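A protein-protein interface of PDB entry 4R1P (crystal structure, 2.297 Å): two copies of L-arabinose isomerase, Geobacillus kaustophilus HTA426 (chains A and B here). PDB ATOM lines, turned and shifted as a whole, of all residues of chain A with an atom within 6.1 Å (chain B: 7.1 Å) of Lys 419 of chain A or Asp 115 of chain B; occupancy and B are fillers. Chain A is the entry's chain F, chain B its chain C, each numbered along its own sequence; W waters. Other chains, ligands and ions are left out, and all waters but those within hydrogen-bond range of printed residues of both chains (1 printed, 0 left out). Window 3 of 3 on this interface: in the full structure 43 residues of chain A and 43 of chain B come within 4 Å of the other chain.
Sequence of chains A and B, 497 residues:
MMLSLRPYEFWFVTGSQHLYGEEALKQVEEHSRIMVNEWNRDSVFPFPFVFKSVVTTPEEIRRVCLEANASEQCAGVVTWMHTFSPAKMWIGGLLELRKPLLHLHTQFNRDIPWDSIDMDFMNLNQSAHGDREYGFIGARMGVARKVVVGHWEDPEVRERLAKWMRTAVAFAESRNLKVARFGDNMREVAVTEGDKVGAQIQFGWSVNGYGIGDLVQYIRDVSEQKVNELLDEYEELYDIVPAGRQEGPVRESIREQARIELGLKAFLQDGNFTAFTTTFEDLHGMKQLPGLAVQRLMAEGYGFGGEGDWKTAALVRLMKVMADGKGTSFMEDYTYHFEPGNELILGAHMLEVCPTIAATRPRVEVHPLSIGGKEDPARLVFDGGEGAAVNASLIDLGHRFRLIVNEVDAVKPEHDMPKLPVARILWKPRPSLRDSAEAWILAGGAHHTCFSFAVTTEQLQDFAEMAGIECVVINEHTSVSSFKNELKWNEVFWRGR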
ATOM      1  N   HIS A 367      11.775  21.157   3.830  1.00  0.00           N
ATOM      2  CA  HIS A 367      12.469  20.405   2.799  1.00  0.00           C
ATOM      3  C   HIS A 367      13.153  21.398   1.886  1.00  0.00           C
ATOM      4  O   HIS A 367      12.789  22.569   1.859  1.00  0.00           O
ATOM      5  CB  HIS A 367      11.501  19.548   1.970  1.00  0.00           C
ATOM      6  CG  HIS A 367      10.784  18.487   2.751  1.00  0.00           C
ATOM      7  ND1 HIS A 367      11.364  17.279   3.079  1.00  0.00           N
ATOM      8  CD2 HIS A 367       9.523  18.443   3.244  1.00  0.00           C
ATOM      9  CE1 HIS A 367      10.495  16.541   3.746  1.00  0.00           C
ATOM     10  NE2 HIS A 367       9.369  17.224   3.861  1.00  0.00           N
ATOM     11  N   HIS A 415      -1.913   4.094  -1.055  1.00  0.00           N
ATOM     12  CA  HIS A 415      -0.495   3.906  -0.787  1.00  0.00           C
ATOM     13  C   HIS A 415       0.097   5.150  -0.156  1.00  0.00           C
ATOM     14  O   HIS A 415      -0.303   6.279  -0.452  1.00  0.00           O
ATOM     15  CB  HIS A 415       0.282   3.608  -2.066  1.00  0.00           C
ATOM     16  CG  HIS A 415      -0.272   2.477  -2.873  1.00  0.00           C
ATOM     17  ND1 HIS A 415      -1.463   2.566  -3.562  1.00  0.00           N
ATOM     18  CD2 HIS A 415       0.217   1.240  -3.126  1.00  0.00           C
ATOM     19  CE1 HIS A 415      -1.691   1.426  -4.192  1.00  0.00           C
ATOM     20  NE2 HIS A 415      -0.685   0.606  -3.945  1.00  0.00           N
ATOM     21  N   ASP A 416       1.075   4.934   0.709  1.00  0.00           N
ATOM     22  CA  ASP A 416       1.767   6.031   1.362  1.00  0.00           C
ATOM     23  C   ASP A 416       2.625   6.728   0.322  1.00  0.00           C
ATOM     24  O   ASP A 416       2.983   6.132  -0.696  1.00  0.00           O
ATOM     25  CB  ASP A 416       2.634   5.496   2.504  1.00  0.00           C
ATOM     26  CG  ASP A 416       3.137   6.590   3.421  1.00  0.00           C
ATOM     27  OD1 ASP A 416       2.312   7.411   3.879  1.00  0.00           O
ATOM     28  OD2 ASP A 416       4.360   6.628   3.675  1.00  0.00           O
ATOM     29  N   MET A 417       2.927   7.999   0.572  1.00  0.00           N
ATOM     30  CA  MET A 417       3.837   8.769  -0.274  1.00  0.00           C
ATOM     31  C   MET A 417       4.852   9.441   0.635  1.00  0.00           C
ATOM     32  O   MET A 417       4.723  10.629   0.950  1.00  0.00           O
ATOM     33  CB  MET A 417       3.070   9.809  -1.108  1.00  0.00           C
ATOM     34  CG  MET A 417       2.427   9.241  -2.374  1.00  0.00           C
ATOM     35  SD  MET A 417       1.191  10.331  -3.125  1.00  0.00           S
ATOM     36  CE  MET A 417      -0.048  10.338  -1.837  1.00  0.00           C
ATOM     37  N   PRO A 418       5.865   8.673   1.070  1.00  0.00           N
ATOM     38  CA  PRO A 418       6.791   9.098   2.123  1.00  0.00           C
ATOM     39  C   PRO A 418       7.855  10.062   1.619  1.00  0.00           C
ATOM     40  O   PRO A 418       8.364  10.870   2.397  1.00  0.00           O
ATOM     41  CB  PRO A 418       7.449   7.783   2.566  1.00  0.00           C
ATOM     42  CG  PRO A 418       7.020   6.733   1.574  1.00  0.00           C
ATOM     43  CD  PRO A 418       6.289   7.403   0.462  1.00  0.00           C
ATOM     44  N   LYS A 419       8.197   9.981   0.339  1.00  0.00           N
ATOM     45  CA  LYS A 419       9.224  10.862  -0.200  1.00  0.00           C
ATOM     46  C   LYS A 419       8.668  12.188  -0.747  1.00  0.00           C
ATOM     47  O   LYS A 419       9.435  13.065  -1.123  1.00  0.00           O
ATOM     48  CB  LYS A 419      10.060  10.131  -1.254  1.00  0.00           C
ATOM     49  CG  LYS A 419      10.886   8.976  -0.692  1.00  0.00           C
ATOM     50  CD  LYS A 419      11.799   9.444   0.438  1.00  0.00           C
ATOM     51  CE  LYS A 419      12.600   8.298   1.051  1.00  0.00           C
ATOM     52  NZ  LYS A 419      13.499   7.647   0.059  1.00  0.00           N
ATOM     53  N   LEU A 420       7.341  12.329  -0.763  1.00  0.00           N
ATOM     54  CA  LEU A 420       6.674  13.500  -1.336  1.00  0.00           C
ATOM     55  C   LEU A 420       6.497  14.641  -0.337  1.00  0.00           C
ATOM     56  O   LEU A 420       5.592  14.612   0.503  1.00  0.00           O
ATOM     57  CB  LEU A 420       5.306  13.113  -1.915  1.00  0.00           C
ATOM     58  CG  LEU A 420       4.519  14.232  -2.615  1.00  0.00           C
ATOM     59  CD1 LEU A 420       5.299  14.795  -3.800  1.00  0.00           C
ATOM     60  CD2 LEU A 420       3.154  13.748  -3.065  1.00  0.00           C
ATOM     61  N   PRO A 421       7.330  15.681  -0.462  1.00  0.00           N
ATOM     62  CA  PRO A 421       7.415  16.761   0.531  1.00  0.00           C
ATOM     63  C   PRO A 421       6.269  17.780   0.510  1.00  0.00           C
ATOM     64  O   PRO A 421       6.347  18.769   1.242  1.00  0.00           O
ATOM     65  CB  PRO A 421       8.725  17.450   0.165  1.00  0.00           C
ATOM     66  CG  PRO A 421       8.849  17.232  -1.303  1.00  0.00           C
ATOM     67  CD  PRO A 421       8.278  15.875  -1.573  1.00  0.00           C
ATOM     68  N   ILE B 112       1.751   6.109 -10.915  1.00  0.00           N
ATOM     69  CA  ILE B 112       2.473   6.876  -9.907  1.00  0.00           C
ATOM     70  C   ILE B 112       3.332   5.937  -9.049  1.00  0.00           C
ATOM     71  O   ILE B 112       2.813   4.992  -8.446  1.00  0.00           O
ATOM     72  CB  ILE B 112       1.504   7.652  -8.990  1.00  0.00           C
ATOM     73  CG1 ILE B 112       0.727   8.706  -9.781  1.00  0.00           C
ATOM     74  CG2 ILE B 112       2.251   8.314  -7.831  1.00  0.00           C
ATOM     75  CD1 ILE B 112      -0.340   9.421  -8.957  1.00  0.00           C
ATOM     76  N   PRO B 113       4.651   6.185  -9.000  1.00  0.00           N
ATOM     77  CA  PRO B 113       5.543   5.443  -8.095  1.00  0.00           C
ATOM     78  C   PRO B 113       5.387   5.936  -6.658  1.00  0.00           C
ATOM     79  O   PRO B 113       6.194   6.740  -6.191  1.00  0.00           O
ATOM     80  CB  PRO B 113       6.934   5.793  -8.621  1.00  0.00           C
ATOM     81  CG  PRO B 113       6.765   7.161  -9.235  1.00  0.00           C
ATOM     82  CD  PRO B 113       5.379   7.167  -9.825  1.00  0.00           C
ATOM     83  N   TRP B 114       4.352   5.457  -5.972  1.00  0.00           N
ATOM     84  CA  TRP B 114       3.979   5.974  -4.655  1.00  0.00           C
ATOM     85  C   TRP B 114       5.128   5.932  -3.652  1.00  0.00           C
ATOM     86  O   TRP B 114       5.225   6.785  -2.767  1.00  0.00           O
ATOM     87  CB  TRP B 114       2.796   5.183  -4.091  1.00  0.00           C
ATOM     88  CG  TRP B 114       1.700   4.945  -5.080  1.00  0.00           C
ATOM     89  CD1 TRP B 114       1.507   3.827  -5.834  1.00  0.00           C
ATOM     90  CD2 TRP B 114       0.639   5.847  -5.418  1.00  0.00           C
ATOM     91  NE1 TRP B 114       0.389   3.971  -6.622  1.00  0.00           N
ATOM     92  CE2 TRP B 114      -0.158   5.207  -6.389  1.00  0.00           C
ATOM     93  CE3 TRP B 114       0.287   7.136  -4.996  1.00  0.00           C
ATOM     94  CZ2 TRP B 114      -1.287   5.810  -6.943  1.00  0.00           C
ATOM     95  CZ3 TRP B 114      -0.833   7.732  -5.544  1.00  0.00           C
ATOM     96  CH2 TRP B 114      -1.606   7.070  -6.508  1.00  0.00           C
ATOM     97  N   ASP B 115       5.985   4.923  -3.789  1.00  0.00           N
ATOM     98  CA  ASP B 115       7.104   4.735  -2.876  1.00  0.00           C
ATOM     99  C   ASP B 115       8.118   5.854  -3.016  1.00  0.00           C
ATOM    100  O   ASP B 115       8.620   6.395  -2.034  1.00  0.00           O
ATOM    101  CB  ASP B 115       7.802   3.402  -3.165  1.00  0.00           C
ATOM    102  CG  ASP B 115       6.957   2.217  -2.797  1.00  0.00           C
ATOM    103  OD1 ASP B 115       7.268   1.102  -3.269  1.00  0.00           O
ATOM    104  OD2 ASP B 115       5.978   2.404  -2.038  1.00  0.00           O
ATOM    105  N   SER B 116       8.408   6.197  -4.260  1.00  0.00           N
ATOM    106  CA  SER B 116       9.570   7.004  -4.564  1.00  0.00           C
ATOM    107  C   SER B 116       9.235   8.417  -5.020  1.00  0.00           C
ATOM    108  O   SER B 116      10.139   9.254  -5.125  1.00  0.00           O
ATOM    109  CB  SER B 116      10.402   6.289  -5.626  1.00  0.00           C
ATOM    110  OG  SER B 116       9.564   5.536  -6.484  1.00  0.00           O
ATOM    111  N   ILE B 117       7.956   8.689  -5.284  1.00  0.00           N
ATOM    112  CA  ILE B 117       7.581   9.989  -5.828  1.00  0.00           C
ATOM    113  C   ILE B 117       8.030  11.122  -4.914  1.00  0.00           C
ATOM    114  O   ILE B 117       7.697  11.163  -3.731  1.00  0.00           O
ATOM    115  CB  ILE B 117       6.076  10.106  -6.208  1.00  0.00           C
ATOM    116  CG1 ILE B 117       5.820  11.459  -6.887  1.00  0.00           C
ATOM    117  CG2 ILE B 117       5.173   9.902  -4.996  1.00  0.00           C
ATOM    118  CD1 ILE B 117       4.477  11.586  -7.602  1.00  0.00           C
ATOM    119  N   ASP B 118       8.848  12.010  -5.467  1.00  0.00           N
ATOM    120  CA  ASP B 118       9.356  13.148  -4.721  1.00  0.00           C
ATOM    121  C   ASP B 118       9.326  14.362  -5.625  1.00  0.00           C
ATOM    122  O   ASP B 118       8.795  14.293  -6.723  1.00  0.00           O
ATOM    123  CB  ASP B 118      10.781  12.883  -4.220  1.00  0.00           C
ATOM    124  CG  ASP B 118      11.730  12.438  -5.334  1.00  0.00           C
ATOM    125  OD1 ASP B 118      11.399  12.608  -6.527  1.00  0.00           O
ATOM    126  OD2 ASP B 118      12.820  11.921  -5.011  1.00  0.00           O
ATOM    127  N   MET B 119       9.926  15.457  -5.174  1.00  0.00           N
ATOM    128  CA  MET B 119       9.842  16.719  -5.892  1.00  0.00           C
ATOM    129  C   MET B 119      10.511  16.659  -7.261  1.00  0.00           C
ATOM    130  O   MET B 119      10.048  17.300  -8.209  1.00  0.00           O
ATOM    131  CB  MET B 119      10.430  17.855  -5.052  1.00  0.00           C
ATOM    132  CG  MET B 119       9.895  19.220  -5.417  1.00  0.00           C
ATOM    133  SD  MET B 119       8.095  19.294  -5.350  1.00  0.00           S
ATOM    134  CE  MET B 119       7.810  20.959  -5.952  1.00  0.00           C
HETATM  135  O   HOH W   1       6.649   9.449  -1.946  1.00  0.00           O
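His 415 of chain A touches Trp 114 of chain B. Met 417 of chain A touches Trp 114 of chain B (CA to O, 3.5 Å). Met 417 of chain A touches Ile 117 of chain B. O of Trp 114 of chain B touches CD of Pro 418 of chain A, at 3.5 Å. Pro 418 of chain A touches Asp 115 of chain B (CD to O, 3.6 Å). Asp 115 of chain B touches Lys 419 of chain A (O to CG, 3.7 Å). Lys 419 of chain A touches Ser 116 of chain B. Ile 117 of chain B touches Lys 419 of chain A (O to C, 3.3 Å). Asp 118 of chain B touches Lys 419 of chain A (CB to O, 3.4 Å). CD of Pro 421 of chain A touches N of Met 119 of chain B, at 3.98 Å.
His 367 of chain A touches none of the printed residues of chain B. Printed residues of chain B within 4 Å of Asp 416 of chain A: Trp 114. Of chain B, only Asp 115, Ser 116, Ile 117 and Asp 118 come within 4 Å of Lys 419 of chain A. Printed residues of chain B within 4 Å of Pro 421 of chain A: Met 119. Ile 112 of chain B touches none of the printed residues of chain A. Asp 115 of chain B touches just these residues of chain A: Pro 418 (3.6 Å) and Lys 419 (3.7 Å). Printed residues of chain A within 4 Å of Ser 116 of chain B: Lys 419 (3.97 Å). The nearest printed residue of chain A that does not touch Trp 114 of chain B is Lys 419 of chain A (5.4 Å).
Water W1 lies within hydrogen-bond range of the backbone carbonyl oxygen of Ile 117 of chain B (2.7 Å), the backbone NH of Lys 419 of chain A (2.8 Å), the backbone carbonyl oxygen of Trp 114 of chain B (3.1 Å) and the backbone NH of Leu 420 of chain A (3.2 Å).
The indole nitrogen of Trp 114 of chain B sits close to the backbone carbonyl oxygen of Ile 112 of chain B (3.2 Å).
The backbone carbonyl oxygen (O) of Ile 117 of chain B sits at hydrogen-bond distance from the backbone NH (N) of Leu 420 of chain A, 3.2 Å away. The backbone carbonyl oxygen of Asp 416 of chain A lies close to the backbone carbonyl oxygen of Trp 114 of chain B (3.1 Å).
Printed residues of chain A that touch a printed residue of chain B: His 415, Asp 416, Met 417, Pro 418, Lys 419, Leu 420 and Pro 421.
No position is printed for both chains. Of the 12 pairs that touch across the chains among the printed residues, none has its exchanged pair printed and touching as well.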
